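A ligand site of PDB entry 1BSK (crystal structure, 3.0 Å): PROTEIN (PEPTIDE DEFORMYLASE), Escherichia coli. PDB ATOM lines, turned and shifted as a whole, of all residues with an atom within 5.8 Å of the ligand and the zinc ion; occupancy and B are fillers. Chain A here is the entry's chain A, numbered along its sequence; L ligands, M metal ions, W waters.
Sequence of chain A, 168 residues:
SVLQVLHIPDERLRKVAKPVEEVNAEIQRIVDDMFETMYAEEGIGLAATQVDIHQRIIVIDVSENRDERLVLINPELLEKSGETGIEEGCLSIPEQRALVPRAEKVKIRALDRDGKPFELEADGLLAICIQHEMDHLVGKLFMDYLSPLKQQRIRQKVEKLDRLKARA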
ATOM      1  N   GLU A  41      21.919  18.250   8.872  1.00  0.00           N
ATOM      2  CA  GLU A  41      22.051  19.561   8.250  1.00  0.00           C
ATOM      3  C   GLU A  41      23.471  20.086   8.182  1.00  0.00           C
ATOM      4  O   GLU A  41      23.702  21.181   7.688  1.00  0.00           O
ATOM      5  CB  GLU A  41      21.178  20.540   8.999  1.00  0.00           C
ATOM      6  CG  GLU A  41      19.808  19.994   9.304  1.00  0.00           C
ATOM      7  CD  GLU A  41      18.839  20.242   8.187  1.00  0.00           C
ATOM      8  OE1 GLU A  41      18.964  19.558   7.154  1.00  0.00           O
ATOM      9  OE2 GLU A  41      17.958  21.121   8.377  1.00  0.00           O
ATOM     10  N   GLU A  42      24.433  19.303   8.677  1.00  0.00           N
ATOM     11  CA  GLU A  42      25.834  19.736   8.663  1.00  0.00           C
ATOM     12  C   GLU A  42      26.105  20.990   9.484  1.00  0.00           C
ATOM     13  O   GLU A  42      26.987  21.803   9.153  1.00  0.00           O
ATOM     14  CB  GLU A  42      26.356  19.922   7.234  1.00  0.00           C
ATOM     15  CG  GLU A  42      26.273  18.659   6.352  1.00  0.00           C
ATOM     16  CD  GLU A  42      27.017  18.816   5.021  1.00  0.00           C
ATOM     17  OE1 GLU A  42      26.406  19.309   4.033  1.00  0.00           O
ATOM     18  OE2 GLU A  42      28.187  18.400   4.968  1.00  0.00           O
ATOM     19  N   GLY A  43      25.316  21.180  10.544  1.00  0.00           N
ATOM     20  CA  GLY A  43      25.513  22.328  11.408  1.00  0.00           C
ATOM     21  C   GLY A  43      26.498  21.955  12.472  1.00  0.00           C
ATOM     22  O   GLY A  43      26.692  20.766  12.730  1.00  0.00           O
ATOM     23  N   ILE A  44      27.145  22.951  13.077  1.00  0.00           N
ATOM     24  CA  ILE A  44      28.110  22.690  14.160  1.00  0.00           C
ATOM     25  C   ILE A  44      27.484  22.829  15.556  1.00  0.00           C
ATOM     26  O   ILE A  44      28.122  22.581  16.578  1.00  0.00           O
ATOM     27  CB  ILE A  44      29.432  23.538  14.022  1.00  0.00           C
ATOM     28  CG1 ILE A  44      29.189  25.021  14.348  1.00  0.00           C
ATOM     29  CG2 ILE A  44      29.979  23.473  12.632  1.00  0.00           C
ATOM     30  CD1 ILE A  44      30.440  25.907  14.230  1.00  0.00           C
ATOM     31  N   GLY A  45      26.224  23.226  15.603  1.00  0.00           N
ATOM     32  CA  GLY A  45      25.531  23.378  16.863  1.00  0.00           C
ATOM     33  C   GLY A  45      24.033  23.452  16.599  1.00  0.00           C
ATOM     34  O   GLY A  45      23.606  23.493  15.438  1.00  0.00           O
ATOM     35  N   LEU A  46      23.240  23.434  17.658  1.00  0.00           N
ATOM     36  CA  LEU A  46      21.776  23.528  17.517  1.00  0.00           C
ATOM     37  C   LEU A  46      21.072  23.817  18.832  1.00  0.00           C
ATOM     38  O   LEU A  46      21.231  23.084  19.812  1.00  0.00           O
ATOM     39  CB  LEU A  46      21.209  22.218  16.931  1.00  0.00           C
ATOM     40  CG  LEU A  46      19.711  22.292  16.607  1.00  0.00           C
ATOM     41  CD1 LEU A  46      19.504  22.996  15.281  1.00  0.00           C
ATOM     42  CD2 LEU A  46      19.132  20.913  16.512  1.00  0.00           C
ATOM     43  N   ALA A  47      20.331  24.905  18.872  1.00  0.00           N
ATOM     44  CA  ALA A  47      19.576  25.272  20.073  1.00  0.00           C
ATOM     45  C   ALA A  47      18.148  24.706  19.975  1.00  0.00           C
ATOM     46  O   ALA A  47      17.547  24.714  18.899  1.00  0.00           O
ATOM     47  CB  ALA A  47      19.535  26.739  20.251  1.00  0.00           C
ATOM     48  N   GLN A  50      15.312  26.368  17.956  1.00  0.00           N
ATOM     49  CA  GLN A  50      15.251  26.243  16.508  1.00  0.00           C
ATOM     50  C   GLN A  50      14.324  25.129  16.049  1.00  0.00           C
ATOM     51  O   GLN A  50      13.735  25.230  14.985  1.00  0.00           O
ATOM     52  CB  GLN A  50      16.644  25.993  15.941  1.00  0.00           C
ATOM     53  CG  GLN A  50      17.622  27.128  16.139  1.00  0.00           C
ATOM     54  CD  GLN A  50      19.005  26.745  15.657  1.00  0.00           C
ATOM     55  OE1 GLN A  50      19.825  26.274  16.423  1.00  0.00           O
ATOM     56  NE2 GLN A  50      19.266  26.947  14.373  1.00  0.00           N
ATOM     57  N   ILE A  86      33.486  35.794  13.230  1.00  0.00           N
ATOM     58  CA  ILE A  86      33.547  34.946  12.048  1.00  0.00           C
ATOM     59  C   ILE A  86      32.278  35.116  11.198  1.00  0.00           C
ATOM     60  O   ILE A  86      31.278  35.685  11.666  1.00  0.00           O
ATOM     61  CB  ILE A  86      33.670  33.447  12.414  1.00  0.00           C
ATOM     62  CG1 ILE A  86      32.411  32.980  13.141  1.00  0.00           C
ATOM     63  CG2 ILE A  86      34.863  33.183  13.315  1.00  0.00           C
ATOM     64  CD1 ILE A  86      32.329  31.495  13.324  1.00  0.00           C
ATOM     65  N   GLU A  87      32.333  34.683   9.942  1.00  0.00           N
ATOM     66  CA  GLU A  87      31.181  34.765   9.056  1.00  0.00           C
ATOM     67  C   GLU A  87      30.215  33.677   9.504  1.00  0.00           C
ATOM     68  O   GLU A  87      30.232  32.553   8.976  1.00  0.00           O
ATOM     69  CB  GLU A  87      31.611  34.553   7.622  1.00  0.00           C
ATOM     70  CG  GLU A  87      32.766  35.440   7.235  1.00  0.00           C
ATOM     71  CD  GLU A  87      32.351  36.548   6.315  1.00  0.00           C
ATOM     72  OE1 GLU A  87      31.598  37.413   6.781  1.00  0.00           O
ATOM     73  OE2 GLU A  87      32.806  36.562   5.155  1.00  0.00           O
ATOM     74  N   GLU A  88      29.368  34.022  10.459  1.00  0.00           N
ATOM     75  CA  GLU A  88      28.410  33.087  10.996  1.00  0.00           C
ATOM     76  C   GLU A  88      27.254  32.799  10.077  1.00  0.00           C
ATOM     77  O   GLU A  88      26.851  33.654   9.287  1.00  0.00           O
ATOM     78  CB  GLU A  88      27.881  33.560  12.338  1.00  0.00           C
ATOM     79  CG  GLU A  88      28.920  33.514  13.438  1.00  0.00           C
ATOM     80  CD  GLU A  88      28.400  34.013  14.756  1.00  0.00           C
ATOM     81  OE1 GLU A  88      27.205  33.839  15.013  1.00  0.00           O
ATOM     82  OE2 GLU A  88      29.194  34.575  15.548  1.00  0.00           O
ATOM     83  N   GLY A  89      26.709  31.598  10.213  1.00  0.00           N
ATOM     84  CA  GLY A  89      25.565  31.175   9.449  1.00  0.00           C
ATOM     85  C   GLY A  89      24.597  30.589  10.438  1.00  0.00           C
ATOM     86  O   GLY A  89      24.955  30.418  11.604  1.00  0.00           O
ATOM     87  N   CYS A  90      23.384  30.283   9.996  1.00  0.00           N
ATOM     88  CA  CYS A  90      22.392  29.700  10.886  1.00  0.00           C
ATOM     89  C   CYS A  90      21.436  28.884  10.017  1.00  0.00           C
ATOM     90  O   CYS A  90      21.146  29.267   8.892  1.00  0.00           O
ATOM     91  CB  CYS A  90      21.663  30.794  11.639  1.00  0.00           C
ATOM     92  SG  CYS A  90      20.529  30.186  12.913  1.00  0.00           S
ATOM     93  N   LEU A  91      20.959  27.759  10.529  1.00  0.00           N
ATOM     94  CA  LEU A  91      20.033  26.940   9.784  1.00  0.00           C
ATOM     95  C   LEU A  91      18.652  27.597   9.746  1.00  0.00           C
ATOM     96  O   LEU A  91      17.772  27.186   8.970  1.00  0.00           O
ATOM     97  CB  LEU A  91      19.928  25.558  10.433  1.00  0.00           C
ATOM     98  CG  LEU A  91      21.154  24.646  10.328  1.00  0.00           C
ATOM     99  CD1 LEU A  91      20.860  23.359  11.067  1.00  0.00           C
ATOM    100  CD2 LEU A  91      21.505  24.354   8.866  1.00  0.00           C
ATOM    101  N   SER A  92      18.463  28.613  10.597  1.00  0.00           N
ATOM    102  CA  SER A  92      17.221  29.382  10.677  1.00  0.00           C
ATOM    103  C   SER A  92      17.260  30.599   9.760  1.00  0.00           C
ATOM    104  O   SER A  92      16.249  31.228   9.490  1.00  0.00           O
ATOM    105  CB  SER A  92      16.924  29.811  12.131  1.00  0.00           C
ATOM    106  OG  SER A  92      16.524  28.706  12.949  1.00  0.00           O
ATOM    107  N   ARG A  97      25.157  34.981   5.723  1.00  0.00           N
ATOM    108  CA  ARG A  97      26.330  34.941   6.596  1.00  0.00           C
ATOM    109  C   ARG A  97      26.747  36.355   6.925  1.00  0.00           C
ATOM    110  O   ARG A  97      26.811  37.207   6.035  1.00  0.00           O
ATOM    111  CB  ARG A  97      27.519  34.275   5.889  1.00  0.00           C
ATOM    112  CG  ARG A  97      27.319  32.853   5.425  1.00  0.00           C
ATOM    113  CD  ARG A  97      27.991  31.836   6.342  1.00  0.00           C
ATOM    114  NE  ARG A  97      27.594  30.469   5.982  1.00  0.00           N
ATOM    115  CZ  ARG A  97      28.408  29.416   6.002  1.00  0.00           C
ATOM    116  NH1 ARG A  97      29.687  29.554   6.335  1.00  0.00           N
ATOM    117  NH2 ARG A  97      27.955  28.233   5.581  1.00  0.00           N
ATOM    118  N   LEU A 125      36.545  28.723  17.959  1.00  0.00           N
ATOM    119  CA  LEU A 125      35.246  28.445  17.374  1.00  0.00           C
ATOM    120  C   LEU A 125      34.281  27.919  18.403  1.00  0.00           C
ATOM    121  O   LEU A 125      33.133  28.290  18.383  1.00  0.00           O
ATOM    122  CB  LEU A 125      35.376  27.461  16.230  1.00  0.00           C
ATOM    123  CG  LEU A 125      34.139  27.149  15.375  1.00  0.00           C
ATOM    124  CD1 LEU A 125      33.823  28.348  14.504  1.00  0.00           C
ATOM    125  CD2 LEU A 125      34.412  25.909  14.520  1.00  0.00           C
ATOM    126  N   ILE A 128      32.756  30.793  20.186  1.00  0.00           N
ATOM    127  CA  ILE A 128      31.828  31.531  19.347  1.00  0.00           C
ATOM    128  C   ILE A 128      30.503  30.761  19.231  1.00  0.00           C
ATOM    129  O   ILE A 128      29.440  31.310  19.529  1.00  0.00           O
ATOM    130  CB  ILE A 128      32.410  31.818  17.953  1.00  0.00           C
ATOM    131  CG1 ILE A 128      33.632  32.756  18.109  1.00  0.00           C
ATOM    132  CG2 ILE A 128      31.352  32.478  17.060  1.00  0.00           C
ATOM    133  CD1 ILE A 128      34.377  33.021  16.837  1.00  0.00           C
ATOM    134  N   CYS A 129      30.579  29.482  18.897  1.00  0.00           N
ATOM    135  CA  CYS A 129      29.411  28.600  18.778  1.00  0.00           C
ATOM    136  C   CYS A 129      28.488  28.711  20.016  1.00  0.00           C
ATOM    137  O   CYS A 129      27.298  28.992  19.861  1.00  0.00           O
ATOM    138  CB  CYS A 129      29.873  27.152  18.581  1.00  0.00           C
ATOM    139  SG  CYS A 129      28.564  26.041  18.061  1.00  0.00           S
ATOM    140  N   HIS A 132      26.628  31.844  20.212  1.00  0.00           N
ATOM    141  CA  HIS A 132      25.590  31.804  19.172  1.00  0.00           C
ATOM    142  C   HIS A 132      24.383  31.007  19.652  1.00  0.00           C
ATOM    143  O   HIS A 132      23.259  31.519  19.621  1.00  0.00           O
ATOM    144  CB  HIS A 132      26.109  31.193  17.842  1.00  0.00           C
ATOM    145  CG  HIS A 132      25.095  31.145  16.739  1.00  0.00           C
ATOM    146  ND1 HIS A 132      25.165  31.912  15.587  1.00  0.00           N
ATOM    147  CD2 HIS A 132      23.983  30.385  16.602  1.00  0.00           C
ATOM    148  CE1 HIS A 132      24.130  31.604  14.817  1.00  0.00           C
ATOM    149  NE2 HIS A 132      23.379  30.676  15.386  1.00  0.00           N
ATOM    150  N   GLU A 133      24.629  29.781  20.077  1.00  0.00           N
ATOM    151  CA  GLU A 133      23.580  28.867  20.571  1.00  0.00           C
ATOM    152  C   GLU A 133      22.834  29.342  21.824  1.00  0.00           C
ATOM    153  O   GLU A 133      21.644  29.017  21.992  1.00  0.00           O
ATOM    154  CB  GLU A 133      24.159  27.466  20.792  1.00  0.00           C
ATOM    155  CG  GLU A 133      24.734  26.830  19.542  1.00  0.00           C
ATOM    156  CD  GLU A 133      23.795  26.869  18.344  1.00  0.00           C
ATOM    157  OE1 GLU A 133      22.570  26.852  18.542  1.00  0.00           O
ATOM    158  OE2 GLU A 133      24.320  26.896  17.214  1.00  0.00           O
ATOM    159  N   HIS A 136      20.248  31.993  20.916  1.00  0.00           N
ATOM    160  CA  HIS A 136      19.088  31.282  20.405  1.00  0.00           C
ATOM    161  C   HIS A 136      18.108  30.957  21.518  1.00  0.00           C
ATOM    162  O   HIS A 136      16.899  30.951  21.300  1.00  0.00           O
ATOM    163  CB  HIS A 136      19.513  29.973  19.756  1.00  0.00           C
ATOM    164  CG  HIS A 136      19.655  30.027  18.278  1.00  0.00           C
ATOM    165  ND1 HIS A 136      18.728  30.643  17.460  1.00  0.00           N
ATOM    166  CD2 HIS A 136      20.613  29.518  17.470  1.00  0.00           C
ATOM    167  CE1 HIS A 136      19.153  30.470  16.223  1.00  0.00           C
ATOM    168  NE2 HIS A 136      20.291  29.796  16.192  1.00  0.00           N
ATOM    169  N   LEU A 141      18.823  36.179  17.507  1.00  0.00           N
ATOM    170  CA  LEU A 141      19.441  35.583  16.313  1.00  0.00           C
ATOM    171  C   LEU A 141      20.654  36.431  15.965  1.00  0.00           C
ATOM    172  O   LEU A 141      20.747  37.579  16.386  1.00  0.00           O
ATOM    173  CB  LEU A 141      18.448  35.567  15.139  1.00  0.00           C
ATOM    174  CG  LEU A 141      17.225  34.692  15.360  1.00  0.00           C
ATOM    175  CD1 LEU A 141      16.106  35.017  14.411  1.00  0.00           C
ATOM    176  CD2 LEU A 141      17.607  33.247  15.210  1.00  0.00           C
ATOM    177  N   PHE A 142      21.577  35.878  15.172  1.00  0.00           N
ATOM    178  CA  PHE A 142      22.788  36.622  14.839  1.00  0.00           C
ATOM    179  C   PHE A 142      22.564  37.909  14.070  1.00  0.00           C
ATOM    180  O   PHE A 142      23.411  38.812  14.118  1.00  0.00           O
ATOM    181  CB  PHE A 142      23.833  35.724  14.132  1.00  0.00           C
ATOM    182  CG  PHE A 142      23.619  35.569  12.655  1.00  0.00           C
ATOM    183  CD1 PHE A 142      23.994  36.568  11.768  1.00  0.00           C
ATOM    184  CD2 PHE A 142      23.077  34.401  12.147  1.00  0.00           C
ATOM    185  CE1 PHE A 142      23.840  36.406  10.387  1.00  0.00           C
ATOM    186  CE2 PHE A 142      22.908  34.237  10.767  1.00  0.00           C
ATOM    187  CZ  PHE A 142      23.296  35.243   9.893  1.00  0.00           C
HETATM  188  O1  LIG L   1      22.331  27.672  15.178  1.00  0.00           O
HETATM  189  P1  LIG L   1      22.679  26.412  14.229  1.00  0.00           P
HETATM  190  O2  LIG L   1      24.452  26.308  14.099  1.00  0.00           O
HETATM  191  O3  LIG L   1      21.868  26.536  12.873  1.00  0.00           O
HETATM  192  C1  LIG L   1      25.051  27.309  13.337  1.00  0.00           C
HETATM  193  C2  LIG L   1      25.762  26.606  12.217  1.00  0.00           C
HETATM  194  C3  LIG L   1      25.852  27.970  14.508  1.00  0.00           C
HETATM  195  C4  LIG L   1      27.383  27.827  14.686  1.00  0.00           C
HETATM  196  C5  LIG L   1      28.253  29.048  15.111  1.00  0.00           C
HETATM  197  C6  LIG L   1      28.075  30.035  13.978  1.00  0.00           C
HETATM  198  O4  LIG L   1      25.918  25.414  12.195  1.00  0.00           O
HETATM  199  N1  LIG L   1      26.188  27.479  11.258  1.00  0.00           N
HETATM  200  C7  LIG L   1      27.014  27.049  10.143  1.00  0.00           C
HETATM  201  C8  LIG L   1      26.202  27.296   8.886  1.00  0.00           C
HETATM  202  C9  LIG L   1      25.026  26.344   8.874  1.00  0.00           C
HETATM  203  C10 LIG L   1      24.115  26.746   7.766  1.00  0.00           C
HETATM  204  C11 LIG L   1      25.380  24.892   8.604  1.00  0.00           C
HETATM  205  C12 LIG L   1      28.258  27.872  10.386  1.00  0.00           C
HETATM  206  N2  LIG L   1      29.602  27.144  10.395  1.00  0.00           N
HETATM  207  O5  LIG L   1      28.182  29.068  10.584  1.00  0.00           O
HETATM  208  C13 LIG L   1      30.771  27.704  10.465  1.00  0.00           C
HETATM  209  C14 LIG L   1      30.979  29.095  10.255  1.00  0.00           C
HETATM  210  C15 LIG L   1      32.300  29.566  10.178  1.00  0.00           C
HETATM  211  C16 LIG L   1      33.379  28.651  10.464  1.00  0.00           C
HETATM  212  C17 LIG L   1      33.176  27.274  10.707  1.00  0.00           C
HETATM  213  C18 LIG L   1      31.833  26.806  10.774  1.00  0.00           C
HETATM  214  N3  LIG L   1      34.707  29.167  10.506  1.00  0.00           N
HETATM  215  O6  LIG L   1      35.722  28.448  10.884  1.00  0.00           O
HETATM  216  O7  LIG L   1      34.877  30.444  10.154  1.00  0.00           O
HETATM  217 ZN    ZN M   1      21.757  29.580  14.745  1.00  0.00          ZN
HETATM  218  O   HOH W   1      21.393  32.888  14.505  1.00  0.00           O
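O of Gly 45 lies close to O2 of the ligand (3.2 Å). Residues that only touch the ligand: Glu 42, Gly 43, Ile 86, Glu 87, Glu 88, Arg 97, Leu 125 and Cys 129. Hydrophobic or aromatic side chains within 4 Å of the ligand: Ile 44, Ile 86, Leu 91, Leu 125, His 132 and His 136. Of the 24 residues printed, 17 come within 4 Å of the ligand. The nearest printed residue that does not touch the ligand is Glu 41 (4.2 Å).
The zinc ion is bound by an oxygen (O1) of the ligand, a ring nitrogen (NE2) of His 132, a ring nitrogen (NE2) of His 136 and the side-chain sulfur (SG) of Cys 90. The zinc ion has four donor atoms within binding distance.
N1 of the ligand is in hydrogen-bond range of O of Gly 89 (3.2 Å). NE2 of Gln 50 lies within hydrogen-bond range of O3 of the ligand, 3.0 Å away. OE2 of Glu 133 sits close to O1 of the ligand (3.0 Å). The backbone NH (N) of Ile 44 lies within hydrogen-bond range of an oxygen (O4) of the ligand (2.9 Å). O5 of the ligand sits at hydrogen-bond distance from N of Gly 89 (3.0 Å). O3 of the ligand sits at hydrogen-bond distance from N of Leu 91.
Gln 50 touches the zinc ion. Of the 24 residues printed, 4 come within 4 Å of the zinc ion. The nearest printed residue that does not touch the zinc ion is Glu 133 (4.5 Å).
The backbone carbonyl oxygen (O) of Ile 44 lies within hydrogen-bond range of the side-chain sulfur (SG) of Cys 129, at 3.8 Å. The side-chain sulfur of Cys 90 sits close to the backbone NH of Ser 92 (3.5 Å). OE1 of Glu 133 lies within hydrogen-bond range of N of Ala 47, 3.0 Å away. The side-chain amide oxygen (OE1) of Gln 50 sits at hydrogen-bond distance from the backbone NH (N) of Ala 47, at 2.9 Å. SG of Cys 90 lies close to NE2 of Gln 50 (3.8 Å). A ring nitrogen (ND1) of His 132 sits at hydrogen-bond distance from the side-chain carboxylate (OE1) of Glu 88 (2.9 Å).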
